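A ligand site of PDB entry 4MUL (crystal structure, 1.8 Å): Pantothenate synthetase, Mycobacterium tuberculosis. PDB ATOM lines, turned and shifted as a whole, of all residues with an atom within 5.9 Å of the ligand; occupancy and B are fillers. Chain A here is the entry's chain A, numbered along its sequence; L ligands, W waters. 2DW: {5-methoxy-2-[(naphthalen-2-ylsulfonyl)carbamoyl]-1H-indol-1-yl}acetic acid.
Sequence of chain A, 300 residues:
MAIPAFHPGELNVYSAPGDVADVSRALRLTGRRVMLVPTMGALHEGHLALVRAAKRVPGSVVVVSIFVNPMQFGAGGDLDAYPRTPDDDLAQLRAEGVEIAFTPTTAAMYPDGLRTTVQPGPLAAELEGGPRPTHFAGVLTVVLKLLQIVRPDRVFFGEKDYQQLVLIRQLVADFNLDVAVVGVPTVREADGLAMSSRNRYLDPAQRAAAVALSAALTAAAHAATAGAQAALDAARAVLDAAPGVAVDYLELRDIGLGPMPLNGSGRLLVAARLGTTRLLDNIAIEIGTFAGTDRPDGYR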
ATOM      1  N   PRO A  38       4.945   7.415   9.328  1.00  0.00           N
ATOM      2  CA  PRO A  38       5.534   6.376  10.214  1.00  0.00           C
ATOM      3  C   PRO A  38       6.899   6.030   9.733  1.00  0.00           C
ATOM      4  O   PRO A  38       7.117   5.794   8.496  1.00  0.00           O
ATOM      5  CB  PRO A  38       4.640   5.160   9.981  1.00  0.00           C
ATOM      6  CG  PRO A  38       3.589   5.576   8.974  1.00  0.00           C
ATOM      7  CD  PRO A  38       4.114   6.777   8.259  1.00  0.00           C
ATOM      8  N   THR A  39       7.830   6.046  10.674  1.00  0.00           N
ATOM      9  CA  THR A  39       9.252   5.771  10.334  1.00  0.00           C
ATOM     10  C   THR A  39       9.842   4.799  11.366  1.00  0.00           C
ATOM     11  O   THR A  39       9.278   4.597  12.427  1.00  0.00           O
ATOM     12  CB  THR A  39      10.084   7.033  10.328  1.00  0.00           C
ATOM     13  OG1 THR A  39      10.388   7.429  11.675  1.00  0.00           O
ATOM     14  CG2 THR A  39       9.287   8.238   9.616  1.00  0.00           C
ATOM     15  N   MET A  40      10.992   4.202  11.001  1.00  0.00           N
ATOM     16  CA  MET A  40      11.787   3.481  12.003  1.00  0.00           C
ATOM     17  C   MET A  40      12.958   4.297  12.394  1.00  0.00           C
ATOM     18  O   MET A  40      13.992   3.760  12.783  1.00  0.00           O
ATOM     19  CB  MET A  40      12.301   2.209  11.443  1.00  0.00           C
ATOM     20  CG  MET A  40      11.236   1.407  11.013  1.00  0.00           C
ATOM     21  SD  MET A  40      11.983  -0.193  10.555  1.00  0.00           S
ATOM     22  CE  MET A  40      10.772  -0.794  11.536  1.00  0.00           C
ATOM     23  N   GLY A  41      12.818   5.608  12.259  1.00  0.00           N
ATOM     24  CA  GLY A  41      13.906   6.508  12.710  1.00  0.00           C
ATOM     25  C   GLY A  41      15.061   6.490  11.699  1.00  0.00           C
ATOM     26  O   GLY A  41      14.909   6.028  10.548  1.00  0.00           O
ATOM     27  N   LEU A  43      16.445   9.194  10.261  1.00  0.00           N
ATOM     28  CA  LEU A  43      15.772   9.960   9.211  1.00  0.00           C
ATOM     29  C   LEU A  43      16.712  10.548   8.205  1.00  0.00           C
ATOM     30  O   LEU A  43      17.786  11.041   8.549  1.00  0.00           O
ATOM     31  CB  LEU A  43      14.918  11.072   9.773  1.00  0.00           C
ATOM     32  CG  LEU A  43      13.845  10.619  10.792  1.00  0.00           C
ATOM     33  CD1 LEU A  43      13.017  11.827  11.156  1.00  0.00           C
ATOM     34  CD2 LEU A  43      12.993   9.491  10.260  1.00  0.00           C
ATOM     35  N   HIS A  44      16.331  10.448   6.950  1.00  0.00           N
ATOM     36  CA  HIS A  44      17.135  11.098   5.910  1.00  0.00           C
ATOM     37  C   HIS A  44      16.200  11.982   5.090  1.00  0.00           C
ATOM     38  O   HIS A  44      15.009  12.083   5.368  1.00  0.00           O
ATOM     39  CB  HIS A  44      17.800  10.014   5.107  1.00  0.00           C
ATOM     40  CG  HIS A  44      16.822   9.033   4.522  1.00  0.00           C
ATOM     41  ND1 HIS A  44      16.815   7.688   4.843  1.00  0.00           N
ATOM     42  CD2 HIS A  44      15.754   9.230   3.719  1.00  0.00           C
ATOM     43  CE1 HIS A  44      15.822   7.091   4.191  1.00  0.00           C
ATOM     44  NE2 HIS A  44      15.159   8.012   3.516  1.00  0.00           N
ATOM     45  N   GLU A  45      16.749  12.650   4.079  1.00  0.00           N
ATOM     46  CA  GLU A  45      16.015  13.491   3.173  1.00  0.00           C
ATOM     47  C   GLU A  45      14.742  12.898   2.581  1.00  0.00           C
ATOM     48  O   GLU A  45      13.821  13.628   2.244  1.00  0.00           O
ATOM     49  CB  GLU A  45      16.945  13.885   2.013  1.00  0.00           C
ATOM     50  CG  GLU A  45      16.369  14.965   1.174  1.00  0.00           C
ATOM     51  CD  GLU A  45      16.350  16.309   1.865  1.00  0.00           C
ATOM     52  OE1 GLU A  45      17.021  16.466   2.935  1.00  0.00           O
ATOM     53  OE2 GLU A  45      15.654  17.215   1.357  1.00  0.00           O
ATOM     54  N   GLY A  46      14.716  11.572   2.384  1.00  0.00           N
ATOM     55  CA  GLY A  46      13.494  10.926   1.890  1.00  0.00           C
ATOM     56  C   GLY A  46      12.338  11.047   2.874  1.00  0.00           C
ATOM     57  O   GLY A  46      11.214  11.369   2.496  1.00  0.00           O
ATOM     58  N   HIS A  47      12.660  10.906   4.167  1.00  0.00           N
ATOM     59  CA  HIS A  47      11.670  11.114   5.204  1.00  0.00           C
ATOM     60  C   HIS A  47      11.257  12.564   5.243  1.00  0.00           C
ATOM     61  O   HIS A  47      10.076  12.884   5.495  1.00  0.00           O
ATOM     62  CB  HIS A  47      12.176  10.681   6.594  1.00  0.00           C
ATOM     63  CG  HIS A  47      12.530   9.236   6.696  1.00  0.00           C
ATOM     64  ND1 HIS A  47      13.842   8.807   6.771  1.00  0.00           N
ATOM     65  CD2 HIS A  47      11.767   8.131   6.759  1.00  0.00           C
ATOM     66  CE1 HIS A  47      13.859   7.485   6.833  1.00  0.00           C
ATOM     67  NE2 HIS A  47      12.615   7.057   6.828  1.00  0.00           N
ATOM     68  N   ALA A  49      11.111  14.551   2.816  1.00  0.00           N
ATOM     69  CA  ALA A  49      10.155  14.648   1.673  1.00  0.00           C
ATOM     70  C   ALA A  49       8.745  14.185   2.075  1.00  0.00           C
ATOM     71  O   ALA A  49       7.742  14.789   1.602  1.00  0.00           O
ATOM     72  CB  ALA A  49      10.611  13.904   0.439  1.00  0.00           C
ATOM     73  N   LEU A  50       8.651  13.119   2.888  1.00  0.00           N
ATOM     74  CA  LEU A  50       7.354  12.641   3.380  1.00  0.00           C
ATOM     75  C   LEU A  50       6.712  13.702   4.246  1.00  0.00           C
ATOM     76  O   LEU A  50       5.506  14.046   4.045  1.00  0.00           O
ATOM     77  CB  LEU A  50       7.489  11.310   4.149  1.00  0.00           C
ATOM     78  CG  LEU A  50       8.140  10.146   3.458  1.00  0.00           C
ATOM     79  CD1 LEU A  50       7.926   8.860   4.327  1.00  0.00           C
ATOM     80  CD2 LEU A  50       7.494   9.914   2.055  1.00  0.00           C
ATOM     81  N   GLN A  72       8.873  -7.219  12.812  1.00  0.00           N
ATOM     82  CA  GLN A  72       9.191  -7.427  11.387  1.00  0.00           C
ATOM     83  C   GLN A  72      10.677  -7.861  11.163  1.00  0.00           C
ATOM     84  O   GLN A  72      11.150  -7.988  10.040  1.00  0.00           O
ATOM     85  CB  GLN A  72       8.888  -6.171  10.558  1.00  0.00           C
ATOM     86  CG  GLN A  72       9.762  -4.952  10.899  1.00  0.00           C
ATOM     87  CD  GLN A  72       9.263  -3.665  10.257  1.00  0.00           C
ATOM     88  OE1 GLN A  72       9.896  -3.145   9.302  1.00  0.00           O
ATOM     89  NE2 GLN A  72       8.113  -3.148  10.753  1.00  0.00           N
ATOM     90  N   TYR A  82      19.976  -2.534  13.500  1.00  0.00           N
ATOM     91  CA  TYR A  82      19.269  -1.442  12.857  1.00  0.00           C
ATOM     92  C   TYR A  82      19.765  -0.049  13.337  1.00  0.00           C
ATOM     93  O   TYR A  82      19.900   0.157  14.552  1.00  0.00           O
ATOM     94  CB  TYR A  82      17.766  -1.584  13.060  1.00  0.00           C
ATOM     95  CG  TYR A  82      17.045  -0.782  12.020  1.00  0.00           C
ATOM     96  CD1 TYR A  82      16.908  -1.279  10.712  1.00  0.00           C
ATOM     97  CD2 TYR A  82      16.537   0.480  12.317  1.00  0.00           C
ATOM     98  CE1 TYR A  82      16.284  -0.522   9.708  1.00  0.00           C
ATOM     99  CE2 TYR A  82      15.906   1.244  11.327  1.00  0.00           C
ATOM    100  CZ  TYR A  82      15.793   0.727  10.033  1.00  0.00           C
ATOM    101  OH  TYR A  82      15.177   1.449   9.051  1.00  0.00           O
ATOM    102  N   VAL A 139       5.181  -5.990   9.711  1.00  0.00           N
ATOM    103  CA  VAL A 139       4.977  -4.628   9.209  1.00  0.00           C
ATOM    104  C   VAL A 139       3.463  -4.289   9.241  1.00  0.00           C
ATOM    105  O   VAL A 139       3.081  -3.265   9.653  1.00  0.00           O
ATOM    106  CB  VAL A 139       5.467  -4.532   7.769  1.00  0.00           C
ATOM    107  CG1 VAL A 139       4.971  -3.185   7.165  1.00  0.00           C
ATOM    108  CG2 VAL A 139       6.996  -4.703   7.642  1.00  0.00           C
ATOM    109  N   VAL A 142       2.192  -3.741  12.859  1.00  0.00           N
ATOM    110  CA  VAL A 142       2.574  -2.461  13.454  1.00  0.00           C
ATOM    111  C   VAL A 142       1.880  -1.250  12.775  1.00  0.00           C
ATOM    112  O   VAL A 142       1.487  -0.308  13.440  1.00  0.00           O
ATOM    113  CB  VAL A 142       4.119  -2.290  13.615  1.00  0.00           C
ATOM    114  CG1 VAL A 142       4.820  -1.841  12.303  1.00  0.00           C
ATOM    115  CG2 VAL A 142       4.393  -1.181  14.732  1.00  0.00           C
ATOM    116  N   VAL A 143       1.738  -1.281  11.446  1.00  0.00           N
ATOM    117  CA  VAL A 143       1.187  -0.136  10.751  1.00  0.00           C
ATOM    118  C   VAL A 143      -0.312  -0.050  11.177  1.00  0.00           C
ATOM    119  O   VAL A 143      -0.819   1.026  11.398  1.00  0.00           O
ATOM    120  CB  VAL A 143       1.312  -0.283   9.233  1.00  0.00           C
ATOM    121  CG1 VAL A 143       0.354   0.781   8.450  1.00  0.00           C
ATOM    122  CG2 VAL A 143       2.794  -0.093   8.802  1.00  0.00           C
ATOM    123  N   PHE A 157       4.045   7.272   2.755  1.00  0.00           N
ATOM    124  CA  PHE A 157       5.135   6.305   2.620  1.00  0.00           C
ATOM    125  C   PHE A 157       5.943   6.646   1.374  1.00  0.00           C
ATOM    126  O   PHE A 157       5.357   7.079   0.318  1.00  0.00           O
ATOM    127  CB  PHE A 157       4.568   4.878   2.482  1.00  0.00           C
ATOM    128  CG  PHE A 157       3.889   4.382   3.738  1.00  0.00           C
ATOM    129  CD1 PHE A 157       4.640   3.803   4.780  1.00  0.00           C
ATOM    130  CD2 PHE A 157       2.514   4.440   3.864  1.00  0.00           C
ATOM    131  CE1 PHE A 157       3.975   3.328   5.927  1.00  0.00           C
ATOM    132  CE2 PHE A 157       1.873   4.006   4.985  1.00  0.00           C
ATOM    133  CZ  PHE A 157       2.555   3.441   6.011  1.00  0.00           C
ATOM    134  N   GLY A 158       7.249   6.328   1.437  1.00  0.00           N
ATOM    135  CA  GLY A 158       8.098   6.403   0.229  1.00  0.00           C
ATOM    136  C   GLY A 158       7.758   5.288  -0.733  1.00  0.00           C
ATOM    137  O   GLY A 158       7.316   4.250  -0.324  1.00  0.00           O
ATOM    138  N   GLU A 159       7.963   5.482  -2.032  1.00  0.00           N
ATOM    139  CA  GLU A 159       7.741   4.409  -3.020  1.00  0.00           C
ATOM    140  C   GLU A 159       8.897   3.408  -3.103  1.00  0.00           C
ATOM    141  O   GLU A 159       8.765   2.403  -3.818  1.00  0.00           O
ATOM    142  CB  GLU A 159       7.524   5.019  -4.416  1.00  0.00           C
ATOM    143  CG  GLU A 159       6.199   5.670  -4.501  1.00  0.00           C
ATOM    144  CD  GLU A 159       5.898   6.250  -5.909  1.00  0.00           C
ATOM    145  OE1 GLU A 159       6.734   6.194  -6.804  1.00  0.00           O
ATOM    146  OE2 GLU A 159       4.803   6.798  -6.051  1.00  0.00           O
ATOM    147  N   LYS A 160      10.013   3.680  -2.447  1.00  0.00           N
ATOM    148  CA  LYS A 160      11.207   2.812  -2.582  1.00  0.00           C
ATOM    149  C   LYS A 160      10.907   1.366  -2.145  1.00  0.00           C
ATOM    150  O   LYS A 160      11.139   0.400  -2.873  1.00  0.00           O
ATOM    151  CB  LYS A 160      12.428   3.324  -1.783  1.00  0.00           C
ATOM    152  CG  LYS A 160      13.739   2.569  -2.303  1.00  0.00           C
ATOM    153  CD  LYS A 160      14.841   2.396  -1.219  1.00  0.00           C
ATOM    154  CE  LYS A 160      14.709   1.007  -0.644  1.00  0.00           C
ATOM    155  NZ  LYS A 160      15.272   0.886   0.726  1.00  0.00           N
ATOM    156  N   ASP A 161      10.239   1.240  -1.014  1.00  0.00           N
ATOM    157  CA  ASP A 161       9.741  -0.081  -0.581  1.00  0.00           C
ATOM    158  C   ASP A 161       8.337  -0.287  -1.129  1.00  0.00           C
ATOM    159  O   ASP A 161       7.330  -0.155  -0.421  1.00  0.00           O
ATOM    160  CB  ASP A 161       9.772  -0.164   0.956  1.00  0.00           C
ATOM    161  CG  ASP A 161      11.204  -0.061   1.507  1.00  0.00           C
ATOM    162  OD1 ASP A 161      11.929  -1.040   1.425  1.00  0.00           O
ATOM    163  OD2 ASP A 161      11.610   1.016   1.974  1.00  0.00           O
ATOM    164  N   GLN A 164       6.027  -3.169   0.086  1.00  0.00           N
ATOM    165  CA  GLN A 164       5.448  -2.793   1.334  1.00  0.00           C
ATOM    166  C   GLN A 164       4.287  -1.800   1.162  1.00  0.00           C
ATOM    167  O   GLN A 164       3.214  -1.926   1.803  1.00  0.00           O
ATOM    168  CB  GLN A 164       6.526  -2.129   2.202  1.00  0.00           C
ATOM    169  CG  GLN A 164       5.976  -1.653   3.529  1.00  0.00           C
ATOM    170  CD  GLN A 164       7.062  -1.067   4.379  1.00  0.00           C
ATOM    171  OE1 GLN A 164       7.828  -1.801   4.993  1.00  0.00           O
ATOM    172  NE2 GLN A 164       7.171   0.255   4.384  1.00  0.00           N
ATOM    173  N   ILE A 168       0.413  -2.317   2.253  1.00  0.00           N
ATOM    174  CA  ILE A 168      -0.322  -1.368   3.076  1.00  0.00           C
ATOM    175  C   ILE A 168      -1.642  -0.877   2.451  1.00  0.00           C
ATOM    176  O   ILE A 168      -2.644  -0.666   3.133  1.00  0.00           O
ATOM    177  CB  ILE A 168       0.616  -0.204   3.520  1.00  0.00           C
ATOM    178  CG1 ILE A 168       1.642  -0.763   4.515  1.00  0.00           C
ATOM    179  CG2 ILE A 168      -0.217   0.923   4.272  1.00  0.00           C
ATOM    180  CD1 ILE A 168       2.881   0.176   4.773  1.00  0.00           C
ATOM    181  N   VAL A 184       4.886   8.589  -1.923  1.00  0.00           N
ATOM    182  CA  VAL A 184       5.715   9.722  -2.348  1.00  0.00           C
ATOM    183  C   VAL A 184       6.910   9.238  -3.163  1.00  0.00           C
ATOM    184  O   VAL A 184       7.593   8.307  -2.717  1.00  0.00           O
ATOM    185  CB  VAL A 184       6.208  10.430  -1.118  1.00  0.00           C
ATOM    186  CG1 VAL A 184       7.207  11.636  -1.406  1.00  0.00           C
ATOM    187  CG2 VAL A 184       4.993  10.948  -0.254  1.00  0.00           C
ATOM    188  N   PRO A 185       7.182   9.880  -4.326  1.00  0.00           N
ATOM    189  CA  PRO A 185       8.324   9.340  -5.140  1.00  0.00           C
ATOM    190  C   PRO A 185       9.634   9.361  -4.368  1.00  0.00           C
ATOM    191  O   PRO A 185       9.910  10.282  -3.576  1.00  0.00           O
ATOM    192  CB  PRO A 185       8.422  10.252  -6.357  1.00  0.00           C
ATOM    193  CG  PRO A 185       6.886  10.782  -6.503  1.00  0.00           C
ATOM    194  CD  PRO A 185       6.498  11.014  -5.009  1.00  0.00           C
ATOM    195  N   THR A 186      10.402   8.334  -4.650  1.00  0.00           N
ATOM    196  CA  THR A 186      11.664   8.087  -3.982  1.00  0.00           C
ATOM    197  C   THR A 186      12.644   9.271  -4.203  1.00  0.00           C
ATOM    198  O   THR A 186      12.937   9.625  -5.354  1.00  0.00           O
ATOM    199  CB  THR A 186      12.241   6.782  -4.568  1.00  0.00           C
ATOM    200  OG1 THR A 186      11.373   5.684  -4.233  1.00  0.00           O
ATOM    201  CG2 THR A 186      13.601   6.496  -3.949  1.00  0.00           C
ATOM    202  N   VAL A 187      13.185   9.801  -3.110  1.00  0.00           N
ATOM    203  CA  VAL A 187      14.255  10.824  -3.190  1.00  0.00           C
ATOM    204  C   VAL A 187      15.568  10.103  -3.427  1.00  0.00           C
ATOM    205  O   VAL A 187      15.749   9.008  -2.901  1.00  0.00           O
ATOM    206  CB  VAL A 187      14.328  11.647  -1.828  1.00  0.00           C
ATOM    207  CG1 VAL A 187      15.540  12.643  -1.847  1.00  0.00           C
ATOM    208  CG2 VAL A 187      13.035  12.451  -1.632  1.00  0.00           C
ATOM    209  N   ALA A 194      18.891   5.476  -4.644  1.00  0.00           N
ATOM    210  CA  ALA A 194      17.690   5.732  -3.833  1.00  0.00           C
ATOM    211  C   ALA A 194      18.126   6.016  -2.406  1.00  0.00           C
ATOM    212  O   ALA A 194      18.967   5.295  -1.899  1.00  0.00           O
ATOM    213  CB  ALA A 194      16.782   4.475  -3.813  1.00  0.00           C
ATOM    214  N   MET A 195      17.552   6.999  -1.749  1.00  0.00           N
ATOM    215  CA  MET A 195      17.898   7.202  -0.318  1.00  0.00           C
ATOM    216  C   MET A 195      17.553   5.982   0.495  1.00  0.00           C
ATOM    217  O   MET A 195      16.549   5.266   0.270  1.00  0.00           O
ATOM    218  CB  MET A 195      17.094   8.425   0.263  1.00  0.00           C
ATOM    219  CG  MET A 195      17.472   9.712  -0.322  1.00  0.00           C
ATOM    220  SD  MET A 195      19.208  10.063   0.056  1.00  0.00           S
ATOM    221  CE  MET A 195      19.258  11.776  -0.542  1.00  0.00           C
ATOM    222  N   SER A 196      18.409   5.683   1.458  1.00  0.00           N
ATOM    223  CA  SER A 196      18.129   4.576   2.338  1.00  0.00           C
ATOM    224  C   SER A 196      19.015   4.633   3.579  1.00  0.00           C
ATOM    225  O   SER A 196      20.213   5.015   3.491  1.00  0.00           O
ATOM    226  CB  SER A 196      18.381   3.232   1.669  1.00  0.00           C
ATOM    227  OG  SER A 196      18.302   2.204   2.656  1.00  0.00           O
ATOM    228  N   SER A 197      18.396   4.237   4.697  1.00  0.00           N
ATOM    229  CA  SER A 197      19.092   4.029   5.967  1.00  0.00           C
ATOM    230  C   SER A 197      20.333   3.214   5.762  1.00  0.00           C
ATOM    231  O   SER A 197      21.358   3.463   6.406  1.00  0.00           O
ATOM    232  CB  SER A 197      18.195   3.309   7.005  1.00  0.00           C
ATOM    233  OG  SER A 197      18.110   1.922   6.737  1.00  0.00           O
ATOM    234  N   ARG A 198      20.239   2.245   4.843  1.00  0.00           N
ATOM    235  CA  ARG A 198      21.262   1.235   4.708  1.00  0.00           C
ATOM    236  C   ARG A 198      22.418   1.642   3.770  1.00  0.00           C
ATOM    237  O   ARG A 198      23.395   0.920   3.675  1.00  0.00           O
ATOM    238  CB  ARG A 198      20.671  -0.085   4.262  1.00  0.00           C
ATOM    239  CG  ARG A 198      19.818  -0.774   5.329  1.00  0.00           C
ATOM    240  CD  ARG A 198      20.058  -2.291   5.259  1.00  0.00           C
ATOM    241  NE  ARG A 198      19.417  -2.895   4.080  1.00  0.00           N
ATOM    242  CZ  ARG A 198      18.390  -3.739   4.125  1.00  0.00           C
ATOM    243  NH1 ARG A 198      17.875  -4.240   3.001  1.00  0.00           N
ATOM    244  NH2 ARG A 198      17.849  -4.083   5.305  1.00  0.00           N
HETATM  245  O   2DW L   1      15.588   2.456   3.011  1.00  0.00           O
HETATM  246  C   2DW L   1      15.024   3.553   3.357  1.00  0.00           C
HETATM  247  OXT 2DW L   1      15.303   4.278   4.300  1.00  0.00           O
HETATM  248  CA  2DW L   1      13.945   3.977   2.444  1.00  0.00           C
HETATM  249  N   2DW L   1      12.966   5.056   2.749  1.00  0.00           N
HETATM  250  CBC 2DW L   1      12.782   6.060   1.865  1.00  0.00           C
HETATM  251  CAN 2DW L   1      13.435   6.348   0.685  1.00  0.00           C
HETATM  252  CAI 2DW L   1      13.044   7.462  -0.073  1.00  0.00           C
HETATM  253  CAW 2DW L   1      12.005   8.278   0.385  1.00  0.00           C
HETATM  254  OAT 2DW L   1      11.710   9.309  -0.477  1.00  0.00           O
HETATM  255  CAA 2DW L   1      10.340   9.843  -0.374  1.00  0.00           C
HETATM  256  CAO 2DW L   1      11.402   7.952   1.633  1.00  0.00           C
HETATM  257  CBB 2DW L   1      11.782   6.842   2.349  1.00  0.00           C
HETATM  258  CAQ 2DW L   1      11.365   6.279   3.536  1.00  0.00           C
HETATM  259  CAY 2DW L   1      12.110   5.158   3.779  1.00  0.00           C
HETATM  260  CAV 2DW L   1      12.088   4.261   4.840  1.00  0.00           C
HETATM  261  OAC 2DW L   1      12.611   3.136   4.805  1.00  0.00           O
HETATM  262  NAS 2DW L   1      11.590   4.714   5.985  1.00  0.00           N
HETATM  263  SBE 2DW L   1      11.508   3.840   7.391  1.00  0.00           S
HETATM  264  OAD 2DW L   1      11.602   4.799   8.524  1.00  0.00           O
HETATM  265  OAE 2DW L   1      12.675   2.933   7.737  1.00  0.00           O
HETATM  266  CAX 2DW L   1      10.146   3.077   7.463  1.00  0.00           C
HETATM  267  CAP 2DW L   1      10.136   1.689   7.650  1.00  0.00           C
HETATM  268  CBA 2DW L   1       8.887   1.060   7.776  1.00  0.00           C
HETATM  269  CAL 2DW L   1       8.842  -0.335   7.953  1.00  0.00           C
HETATM  270  CAH 2DW L   1       7.599  -0.913   8.062  1.00  0.00           C
HETATM  271  CAG 2DW L   1       6.404  -0.167   7.990  1.00  0.00           C
HETATM  272  CAK 2DW L   1       6.442   1.205   7.807  1.00  0.00           C
HETATM  273  CAZ 2DW L   1       7.698   1.812   7.710  1.00  0.00           C
HETATM  274  CAM 2DW L   1       7.749   3.185   7.484  1.00  0.00           C
HETATM  275  CAJ 2DW L   1       8.987   3.817   7.380  1.00  0.00           C
HETATM  276  O   HOH W   1       8.112   5.140   3.948  1.00  0.00           O
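The side-chain hydroxyl of Ser 196 is in hydrogen-bond range of an oxygen (O) of the ligand, at 2.7 Å.
The backbone NH of Ser 197 lies within hydrogen-bond range of an oxygen (OXT) of the ligand (3.1 Å).
N of Val 187 is in hydrogen-bond range of OAT of the ligand (3.1 Å).
OAD of the ligand lies within hydrogen-bond range of N of Met 40, at 2.6 Å.
A nitrogen (NAS) of the ligand is in hydrogen-bond range of a ring nitrogen (NE2) of His 47.
O of the ligand is in salt-bridge range of NZ of Lys 160 (2.8 Å).
The side-chain hydroxyl (OH) of Tyr 82 lies within hydrogen-bond range of an oxygen (OAE) of the ligand (3.2 Å).
The backbone carbonyl oxygen (O) of Val 187 lies within hydrogen-bond range of the backbone NH (N) of Met 195, at 2.9 Å.
OG1 of Thr 39 lies within hydrogen-bond range of N of Gly 41 (3.1 Å).
ND1 of His 47 sits at hydrogen-bond distance from N of His 44.
O of Phe 157 is in hydrogen-bond range of N of Val 184 (2.7 Å).
The side-chain carboxylate (OD2) of Asp 161 is in salt-bridge range of the side-chain amino group (NZ) of Lys 160 (3.9 Å).
The backbone NH (N) of Lys 160 sits at hydrogen-bond distance from the side-chain hydroxyl (OG1) of Thr 186 (3.0 Å).
O of Val 184 lies within hydrogen-bond range of N of Glu 159 (2.9 Å).
N of Arg 198 sits at hydrogen-bond distance from OG of Ser 196 (2.9 Å).
Pro 38 touches the ligand.
CA of Thr 39 touches OAD of the ligand, at 3.1 Å.
His 44 touches the ligand.
Gly 46 touches the ligand.
CD2 of Leu 50 touches CAA of the ligand, at 3.7 Å.
OE1 of Gln 72 touches CAL of the ligand, at 3.3 Å.
Val 139 touches the ligand (CG1 to CAG, 3.4 Å).
Val 143 touches the ligand.
Phe 157 touches the ligand.
Gly 158 touches the ligand (CA to CAO, 3.9 Å).
Asp 161 touches the ligand.
Gln 164 touches the ligand (OE1 to CAH, 3.2 Å).
Val 184 touches the ligand (CG1 to CAA, 3.8 Å).
O of Pro 185 touches CAA of the ligand, at 3.3 Å.
CA of Thr 186 touches OAT of the ligand (3.7 Å).
Met 195 touches the ligand.
Hydrophobic or aromatic side chains within 4 Å of the ligand: Met 40, His 44, His 47, Leu 50, Val 139, Val 143, Phe 157, Val 184 and Val 187.
Of the 32 residues printed, 23 come within 4 Å of the ligand.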
